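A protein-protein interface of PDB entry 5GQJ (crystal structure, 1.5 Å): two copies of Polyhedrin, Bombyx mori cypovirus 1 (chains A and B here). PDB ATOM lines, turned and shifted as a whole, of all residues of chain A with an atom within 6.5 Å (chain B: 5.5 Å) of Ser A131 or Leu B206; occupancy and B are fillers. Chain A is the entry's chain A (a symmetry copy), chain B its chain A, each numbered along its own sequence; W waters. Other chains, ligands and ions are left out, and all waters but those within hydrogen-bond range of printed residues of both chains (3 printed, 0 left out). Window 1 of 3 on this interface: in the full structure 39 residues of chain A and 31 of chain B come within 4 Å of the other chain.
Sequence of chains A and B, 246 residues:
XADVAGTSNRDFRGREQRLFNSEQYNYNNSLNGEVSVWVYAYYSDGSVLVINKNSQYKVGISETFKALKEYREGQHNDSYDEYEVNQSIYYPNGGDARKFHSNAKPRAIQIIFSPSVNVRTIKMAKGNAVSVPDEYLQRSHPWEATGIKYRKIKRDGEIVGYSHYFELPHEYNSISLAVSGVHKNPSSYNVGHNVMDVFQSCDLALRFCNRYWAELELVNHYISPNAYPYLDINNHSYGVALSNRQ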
ATOM      1  N   SER A  62      27.581  -7.160  -6.098  1.00  0.00           N
ATOM      2  CA  SER A  62      27.082  -7.339  -7.467  1.00  0.00           C
ATOM      3  C   SER A  62      25.583  -7.147  -7.446  1.00  0.00           C
ATOM      4  O   SER A  62      24.907  -7.831  -6.693  1.00  0.00           O
ATOM      5  CB  SER A  62      27.439  -8.754  -8.023  1.00  0.00           C
ATOM      6  OG  SER A  62      26.823  -8.878  -9.309  1.00  0.00           O
ATOM      7  N   GLU A  63      25.097  -6.220  -8.251  1.00  0.00           N
ATOM      8  CA  GLU A  63      23.659  -5.927  -8.288  1.00  0.00           C
ATOM      9  C   GLU A  63      23.129  -5.813  -9.741  1.00  0.00           C
ATOM     10  O   GLU A  63      23.847  -5.363 -10.672  1.00  0.00           O
ATOM     11  CB  GLU A  63      23.350  -4.640  -7.528  1.00  0.00           C
ATOM     12  CG  GLU A  63      23.838  -4.656  -6.045  1.00  0.00           C
ATOM     13  CD  GLU A  63      23.014  -5.590  -5.150  1.00  0.00           C
ATOM     14  OE1 GLU A  63      21.847  -5.973  -5.530  1.00  0.00           O
ATOM     15  OE2 GLU A  63      23.558  -5.976  -4.072  1.00  0.00           O
ATOM     16  N   THR A  64      21.865  -6.178  -9.885  1.00  0.00           N
ATOM     17  CA  THR A  64      21.131  -6.055 -11.173  1.00  0.00           C
ATOM     18  C   THR A  64      20.763  -4.600 -11.380  1.00  0.00           C
ATOM     19  O   THR A  64      20.776  -3.761 -10.411  1.00  0.00           O
ATOM     20  CB  THR A  64      19.848  -6.900 -11.158  1.00  0.00           C
ATOM     21  OG1 THR A  64      18.920  -6.386 -10.183  1.00  0.00           O
ATOM     22  CG2 THR A  64      20.155  -8.406 -10.929  1.00  0.00           C
ATOM     23  N   PHE A  65      20.362  -4.305 -12.624  1.00  0.00           N
ATOM     24  CA  PHE A  65      19.772  -2.989 -12.931  1.00  0.00           C
ATOM     25  C   PHE A  65      18.558  -2.703 -12.027  1.00  0.00           C
ATOM     26  O   PHE A  65      18.400  -1.582 -11.477  1.00  0.00           O
ATOM     27  CB  PHE A  65      19.356  -2.938 -14.432  1.00  0.00           C
ATOM     28  CG  PHE A  65      18.417  -1.766 -14.734  1.00  0.00           C
ATOM     29  CD1 PHE A  65      18.944  -0.471 -14.931  1.00  0.00           C
ATOM     30  CD2 PHE A  65      17.022  -1.943 -14.752  1.00  0.00           C
ATOM     31  CE1 PHE A  65      18.100   0.617 -15.136  1.00  0.00           C
ATOM     32  CE2 PHE A  65      16.151  -0.819 -14.968  1.00  0.00           C
ATOM     33  CZ  PHE A  65      16.705   0.451 -15.162  1.00  0.00           C
ATOM     34  N   ALA A 125      32.744  -4.541 -13.125  1.00  0.00           N
ATOM     35  CA  ALA A 125      31.929  -4.960 -14.256  1.00  0.00           C
ATOM     36  C   ALA A 125      30.712  -4.011 -14.297  1.00  0.00           C
ATOM     37  O   ALA A 125      29.753  -4.152 -13.527  1.00  0.00           O
ATOM     38  CB  ALA A 125      31.493  -6.438 -14.075  1.00  0.00           C
ATOM     39  N   LYS A 126      30.785  -3.021 -15.170  1.00  0.00           N
ATOM     40  CA  LYS A 126      29.648  -2.097 -15.311  1.00  0.00           C
ATOM     41  C   LYS A 126      28.976  -2.564 -16.546  1.00  0.00           C
ATOM     42  O   LYS A 126      29.438  -2.289 -17.683  1.00  0.00           O
ATOM     43  CB  LYS A 126      30.167  -0.641 -15.356  1.00  0.00           C
ATOM     44  CG  LYS A 126      29.097   0.374 -15.706  1.00  0.00           C
ATOM     45  CD  LYS A 126      29.579   1.812 -15.564  1.00  0.00           C
ATOM     46  CE  LYS A 126      30.571   2.251 -16.621  1.00  0.00           C
ATOM     47  NZ  LYS A 126      29.893   2.668 -17.870  1.00  0.00           N
ATOM     48  N   GLY A 127      27.870  -3.294 -16.342  1.00  0.00           N
ATOM     49  CA  GLY A 127      27.155  -3.906 -17.440  1.00  0.00           C
ATOM     50  C   GLY A 127      26.010  -3.030 -17.980  1.00  0.00           C
ATOM     51  O   GLY A 127      25.673  -1.987 -17.389  1.00  0.00           O
ATOM     52  N   ASN A 128      25.467  -3.428 -19.118  1.00  0.00           N
ATOM     53  CA  ASN A 128      24.227  -2.777 -19.578  1.00  0.00           C
ATOM     54  C   ASN A 128      23.018  -3.315 -18.741  1.00  0.00           C
ATOM     55  O   ASN A 128      23.198  -4.051 -17.739  1.00  0.00           O
ATOM     56  CB  ASN A 128      24.022  -2.978 -21.101  1.00  0.00           C
ATOM     57  CG  ASN A 128      23.786  -4.447 -21.491  1.00  0.00           C
ATOM     58  OD1 ASN A 128      23.546  -5.347 -20.638  1.00  0.00           O
ATOM     59  ND2 ASN A 128      23.870  -4.697 -22.782  1.00  0.00           N
ATOM     60  N   ALA A 129      21.815  -2.907 -19.110  1.00  0.00           N
ATOM     61  CA  ALA A 129      20.651  -3.160 -18.267  1.00  0.00           C
ATOM     62  C   ALA A 129      20.291  -4.645 -18.246  1.00  0.00           C
ATOM     63  O   ALA A 129      19.598  -5.111 -17.318  1.00  0.00           O
ATOM     64  CB  ALA A 129      19.463  -2.311 -18.720  1.00  0.00           C
ATOM     65  N   VAL A 130      20.857  -5.409 -19.183  1.00  0.00           N
ATOM     66  CA  VAL A 130      20.651  -6.895 -19.203  1.00  0.00           C
ATOM     67  C   VAL A 130      21.877  -7.636 -18.739  1.00  0.00           C
ATOM     68  O   VAL A 130      22.010  -8.822 -18.970  1.00  0.00           O
ATOM     69  CB  VAL A 130      20.124  -7.437 -20.594  1.00  0.00           C
ATOM     70  CG1 VAL A 130      18.701  -6.896 -20.846  1.00  0.00           C
ATOM     71  CG2 VAL A 130      21.073  -7.118 -21.795  1.00  0.00           C
ATOM     72  N   SER A 131      22.807  -6.922 -18.098  1.00  0.00           N
ATOM     73  CA  SER A 131      23.858  -7.590 -17.293  1.00  0.00           C
ATOM     74  C   SER A 131      24.966  -8.176 -18.190  1.00  0.00           C
ATOM     75  O   SER A 131      25.560  -9.193 -17.853  1.00  0.00           O
ATOM     76  CB  SER A 131      23.287  -8.646 -16.324  1.00  0.00           C
ATOM     77  OG  SER A 131      22.385  -7.957 -15.405  1.00  0.00           O
ATOM     78  N   VAL A 132      25.249  -7.480 -19.302  1.00  0.00           N
ATOM     79  CA  VAL A 132      26.378  -7.817 -20.209  1.00  0.00           C
ATOM     80  C   VAL A 132      27.433  -6.704 -20.079  1.00  0.00           C
ATOM     81  O   VAL A 132      27.089  -5.516 -20.167  1.00  0.00           O
ATOM     82  CB  VAL A 132      25.868  -7.934 -21.671  1.00  0.00           C
ATOM     83  CG1 VAL A 132      27.023  -8.142 -22.655  1.00  0.00           C
ATOM     84  CG2 VAL A 132      24.864  -9.089 -21.752  1.00  0.00           C
ATOM     85  N   PRO A 133      28.699  -7.108 -19.798  1.00  0.00           N
ATOM     86  CA  PRO A 133      29.738  -6.094 -19.557  1.00  0.00           C
ATOM     87  C   PRO A 133      30.031  -5.160 -20.699  1.00  0.00           C
ATOM     88  O   PRO A 133      30.310  -3.947 -20.448  1.00  0.00           O
ATOM     89  CB  PRO A 133      30.986  -6.950 -19.262  1.00  0.00           C
ATOM     90  CG  PRO A 133      30.445  -8.199 -18.605  1.00  0.00           C
ATOM     91  CD  PRO A 133      29.153  -8.476 -19.405  1.00  0.00           C
ATOM     92  N   LEU A 137      28.046 -10.692 -24.963  1.00  0.00           N
ATOM     93  CA  LEU A 137      28.893 -11.557 -24.156  1.00  0.00           C
ATOM     94  C   LEU A 137      30.146 -12.038 -24.835  1.00  0.00           C
ATOM     95  O   LEU A 137      31.241 -12.137 -24.200  1.00  0.00           O
ATOM     96  CB  LEU A 137      28.114 -12.786 -23.651  1.00  0.00           C
ATOM     97  CG  LEU A 137      26.990 -12.413 -22.641  1.00  0.00           C
ATOM     98  CD1 LEU A 137      26.148 -13.671 -22.405  1.00  0.00           C
ATOM     99  CD2 LEU A 137      27.613 -12.021 -21.290  1.00  0.00           C
ATOM    100  N   PRO A 142      35.271  -9.715 -18.664  1.00  0.00           N
ATOM    101  CA  PRO A 142      34.255  -9.633 -17.622  1.00  0.00           C
ATOM    102  C   PRO A 142      34.478  -8.538 -16.581  1.00  0.00           C
ATOM    103  O   PRO A 142      33.684  -8.412 -15.681  1.00  0.00           O
ATOM    104  CB  PRO A 142      34.329 -11.028 -16.962  1.00  0.00           C
ATOM    105  CG  PRO A 142      34.734 -11.902 -18.091  1.00  0.00           C
ATOM    106  CD  PRO A 142      35.862 -11.076 -18.703  1.00  0.00           C
ATOM    107  N   SER A 176      23.902  -2.335 -14.880  1.00  0.00           N
ATOM    108  CA  SER A 176      24.035  -3.369 -13.822  1.00  0.00           C
ATOM    109  C   SER A 176      25.476  -3.177 -13.339  1.00  0.00           C
ATOM    110  O   SER A 176      26.266  -2.546 -14.019  1.00  0.00           O
ATOM    111  CB  SER A 176      23.822  -4.748 -14.468  1.00  0.00           C
ATOM    112  OG  SER A 176      24.687  -4.893 -15.601  1.00  0.00           O
ATOM    113  N   LEU A 177      25.809  -3.620 -12.118  1.00  0.00           N
ATOM    114  CA  LEU A 177      27.108  -3.248 -11.574  1.00  0.00           C
ATOM    115  C   LEU A 177      27.644  -4.301 -10.598  1.00  0.00           C
ATOM    116  O   LEU A 177      26.954  -4.688  -9.650  1.00  0.00           O
ATOM    117  CB  LEU A 177      26.936  -1.900 -10.809  1.00  0.00           C
ATOM    118  CG  LEU A 177      28.223  -1.349 -10.189  1.00  0.00           C
ATOM    119  CD1 LEU A 177      29.271  -1.073 -11.265  1.00  0.00           C
ATOM    120  CD2 LEU A 177      27.908  -0.094  -9.395  1.00  0.00           C
ATOM    121  N   ALA A 178      28.918  -4.622 -10.783  1.00  0.00           N
ATOM    122  CA  ALA A 178      29.665  -5.369  -9.784  1.00  0.00           C
ATOM    123  C   ALA A 178      31.042  -4.816  -9.610  1.00  0.00           C
ATOM    124  O   ALA A 178      31.647  -4.287 -10.571  1.00  0.00           O
ATOM    125  CB  ALA A 178      29.719  -6.890 -10.155  1.00  0.00           C
ATOM    126  N   ASN B  52      19.749 -15.231 -15.455  1.00  0.00           N
ATOM    127  CA  ASN B  52      21.018 -15.416 -16.136  1.00  0.00           C
ATOM    128  C   ASN B  52      22.168 -14.999 -15.225  1.00  0.00           C
ATOM    129  O   ASN B  52      22.076 -13.998 -14.487  1.00  0.00           O
ATOM    130  CB  ASN B  52      20.946 -14.559 -17.412  1.00  0.00           C
ATOM    131  CG  ASN B  52      22.287 -14.303 -18.084  1.00  0.00           C
ATOM    132  OD1 ASN B  52      22.544 -13.140 -18.439  1.00  0.00           O
ATOM    133  ND2 ASN B  52      23.098 -15.337 -18.371  1.00  0.00           N
ATOM    134  N   LYS B  53      23.288 -15.717 -15.308  1.00  0.00           N
ATOM    135  CA  LYS B  53      24.524 -15.247 -14.656  1.00  0.00           C
ATOM    136  C   LYS B  53      25.637 -15.350 -15.681  1.00  0.00           C
ATOM    137  O   LYS B  53      25.767 -16.349 -16.402  1.00  0.00           O
ATOM    138  CB  LYS B  53      24.829 -16.159 -13.429  1.00  0.00           C
ATOM    139  CG  LYS B  53      26.010 -15.763 -12.582  1.00  0.00           C
ATOM    140  CD  LYS B  53      25.782 -15.128 -11.186  1.00  0.00           C
ATOM    141  CE  LYS B  53      24.764 -15.748 -10.258  1.00  0.00           C
ATOM    142  NZ  LYS B  53      25.578 -16.455  -9.246  1.00  0.00           N
ATOM    143  N   ASN B  54      26.497 -14.330 -15.687  1.00  0.00           N
ATOM    144  CA  ASN B  54      27.636 -14.253 -16.618  1.00  0.00           C
ATOM    145  C   ASN B  54      28.909 -13.993 -15.835  1.00  0.00           C
ATOM    146  O   ASN B  54      28.991 -12.969 -15.098  1.00  0.00           O
ATOM    147  CB  ASN B  54      27.411 -13.081 -17.594  1.00  0.00           C
ATOM    148  CG  ASN B  54      26.091 -13.216 -18.342  1.00  0.00           C
ATOM    149  OD1 ASN B  54      25.827 -14.272 -18.931  1.00  0.00           O
ATOM    150  ND2 ASN B  54      25.269 -12.199 -18.294  1.00  0.00           N
ATOM    151  N   SER B  55      29.900 -14.872 -15.936  1.00  0.00           N
ATOM    152  CA  SER B  55      31.141 -14.634 -15.159  1.00  0.00           C
ATOM    153  C   SER B  55      32.341 -15.254 -15.887  1.00  0.00           C
ATOM    154  O   SER B  55      32.202 -16.192 -16.722  1.00  0.00           O
ATOM    155  CB  SER B  55      30.988 -15.311 -13.796  1.00  0.00           C
ATOM    156  OG  SER B  55      31.895 -14.690 -12.848  1.00  0.00           O
ATOM    157  N   LEU B 204      32.321 -10.573  -9.152  1.00  0.00           N
ATOM    158  CA  LEU B 204      32.152  -9.788 -10.391  1.00  0.00           C
ATOM    159  C   LEU B 204      31.051 -10.314 -11.320  1.00  0.00           C
ATOM    160  O   LEU B 204      30.625  -9.613 -12.240  1.00  0.00           O
ATOM    161  CB  LEU B 204      33.485  -9.728 -11.144  1.00  0.00           C
ATOM    162  CG  LEU B 204      34.526  -8.809 -10.466  1.00  0.00           C
ATOM    163  CD1 LEU B 204      35.962  -9.122 -10.965  1.00  0.00           C
ATOM    164  CD2 LEU B 204      34.207  -7.310 -10.554  1.00  0.00           C
ATOM    165  N   ALA B 205      30.613 -11.543 -11.007  1.00  0.00           N
ATOM    166  CA  ALA B 205      29.603 -12.224 -11.864  1.00  0.00           C
ATOM    167  C   ALA B 205      28.403 -11.287 -11.899  1.00  0.00           C
ATOM    168  O   ALA B 205      27.967 -10.810 -10.858  1.00  0.00           O
ATOM    169  CB  ALA B 205      29.260 -13.605 -11.340  1.00  0.00           C
ATOM    170  N   LEU B 206      27.864 -11.046 -13.090  1.00  0.00           N
ATOM    171  CA  LEU B 206      26.636 -10.227 -13.220  1.00  0.00           C
ATOM    172  C   LEU B 206      25.400 -11.097 -13.346  1.00  0.00           C
ATOM    173  O   LEU B 206      25.453 -12.150 -14.025  1.00  0.00           O
ATOM    174  CB  LEU B 206      26.744  -9.325 -14.435  1.00  0.00           C
ATOM    175  CG  LEU B 206      27.782  -8.180 -14.374  1.00  0.00           C
ATOM    176  CD1 LEU B 206      27.862  -7.423 -15.713  1.00  0.00           C
ATOM    177  CD2 LEU B 206      27.517  -7.213 -13.211  1.00  0.00           C
ATOM    178  N   ARG B 207      24.332 -10.717 -12.647  1.00  0.00           N
ATOM    179  CA  ARG B 207      23.139 -11.538 -12.608  1.00  0.00           C
ATOM    180  C   ARG B 207      21.999 -10.754 -13.317  1.00  0.00           C
ATOM    181  O   ARG B 207      21.996  -9.509 -13.328  1.00  0.00           O
ATOM    182  CB  ARG B 207      22.807 -11.844 -11.154  1.00  0.00           C
ATOM    183  CG  ARG B 207      21.495 -12.618 -10.948  1.00  0.00           C
ATOM    184  CD  ARG B 207      21.297 -13.014  -9.482  1.00  0.00           C
ATOM    185  NE  ARG B 207      20.130 -13.903  -9.278  1.00  0.00           N
ATOM    186  CZ  ARG B 207      18.886 -13.453  -9.162  1.00  0.00           C
ATOM    187  NH1 ARG B 207      18.666 -12.139  -9.260  1.00  0.00           N
ATOM    188  NH2 ARG B 207      17.873 -14.295  -8.951  1.00  0.00           N
ATOM    189  N   PHE B 208      21.042 -11.453 -13.937  1.00  0.00           N
ATOM    190  CA  PHE B 208      19.866 -10.743 -14.502  1.00  0.00           C
ATOM    191  C   PHE B 208      18.664 -11.666 -14.231  1.00  0.00           C
ATOM    192  O   PHE B 208      18.759 -12.930 -14.364  1.00  0.00           O
ATOM    193  CB  PHE B 208      20.041 -10.548 -15.996  1.00  0.00           C
ATOM    194  CG  PHE B 208      18.789 -10.083 -16.728  1.00  0.00           C
ATOM    195  CD1 PHE B 208      18.479  -8.698 -16.777  1.00  0.00           C
ATOM    196  CD2 PHE B 208      17.876 -11.033 -17.283  1.00  0.00           C
ATOM    197  CE1 PHE B 208      17.348  -8.271 -17.474  1.00  0.00           C
ATOM    198  CE2 PHE B 208      16.731 -10.576 -18.013  1.00  0.00           C
ATOM    199  CZ  PHE B 208      16.474  -9.181 -18.052  1.00  0.00           C
HETATM  200  O   HOH W   1      24.542  -8.450 -10.890  1.00  0.00           O
HETATM  201  O   HOH W   2      21.128 -11.329 -19.740  1.00  0.00           O
HETATM  202  O   HOH W   3      32.003 -10.218 -14.576  1.00  0.00           O
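Of the 9 printed residues of chain B, 6 touch a printed residue of chain A.
Hydrophobic or aromatic side chains of chain B within 4 Å of the printed part of chain A: Leu B204, Leu B206 and Phe B208.
Printed residues of chain A that touch a printed residue of chain B: Ser A62, Thr A64, Ala A125, Gly A127, Ala A129, Val A130, Ser A131, Pro A133, Leu A137, Leu A177 and Ala A178.
Among the printed residues, no Asp or Glu carboxylate lies within 4 Å of a Lys or Arg side-chain nitrogen of the other chain.
No position is printed for both chains.
Of the 16 pairs that touch across the chains among the printed residues, none has its exchanged pair printed and touching as well.
The side-chain amide nitrogen of Asn B54 sits at hydrogen-bond distance from the side-chain amide oxygen of Asn B52 (2.9 Å).
The backbone NH (N) of Asn B54 is in hydrogen-bond range of the backbone carbonyl oxygen (O) of Leu B206 (2.9 Å).
The backbone NH of Glu A63 is in hydrogen-bond range of the backbone carbonyl oxygen of Leu A177 (2.8 Å).
The backbone NH (N) of Ala A125 is in hydrogen-bond range of the backbone carbonyl oxygen (O) of Ala A178 (2.8 Å).
N of Gly A127 is in hydrogen-bond range of O of Ser A176.
OD1 of Asn A128 sits close to N of Val A130 (3.1 Å).
O of Ser A131 sits at hydrogen-bond distance from ND2 of Asn B54 (3.1 Å).
The side-chain hydroxyl of Ser A62 lies within hydrogen-bond range of the backbone carbonyl oxygen of Ala B205, at 2.7 Å.
O of Arg B207 sits at hydrogen-bond distance from OG of Ser A131, 2.6 Å away.
Water W2 lies within hydrogen-bond range of the side-chain amide oxygen of Asn B52 (2.6 Å) and the backbone carbonyl oxygen of Val A130 (2.8 Å).
Water W3 bridges O of Pro A142 (2.7 Å) and O of Leu B204 (2.8 Å).
Water W1 lies within hydrogen-bond range of the side-chain hydroxyl of Ser A62, the backbone NH of Arg B207 and the backbone carbonyl oxygen of Glu A63.
Among the printed residues, pairs that only touch across the chains: Thr A64 with Arg B207 (3.2 Å), Leu A137 with Asn B54 (3.5 Å), Ser A131 with Phe B208 (3.5 Å), Ala A178 with Leu B204 (3.5 Å), Ser A131 with Leu B206 (3.6 Å), Val A130 with Phe B208 (3.7 Å), Ala A125 with Leu B204 (3.8 Å), Ala A178 with Leu B206 (3.8 Å), Ala A129 with Phe B208 (3.8 Å), Ala A125 with Leu B206 (3.8 Å), Leu A177 with Leu B206 (3.9 Å), Pro A133 with Leu B206 (3.95 Å) and Gly A127 with Leu B206 (3.98 Å).
Ser A131 touches just these residues of chain B: Asn B54 (3.1 Å), Leu B206 (3.6 Å), Arg B207 (2.6 Å) and Phe B208 (3.5 Å).
Printed residues of chain B within 4 Å of Leu A177: Leu B206 (3.9 Å).
Printed residues of chain B within 4 Å of Ala A178: Leu B204 and Leu B206.
Printed residues of chain A within 4 Å of Arg B207: Thr A64 and Ser A131.
Printed residues of chain A within 4 Å of Phe B208: Ala A129 (3.8 Å), Val A130 (3.7 Å) and Ser A131 (3.5 Å).
The nearest residue of chain B that does not touch Ser A131 is Asn B52 (5.0 Å).
The nearest printed residue of chain A that does not touch Leu B206 is Ser A176 (4.1 Å).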
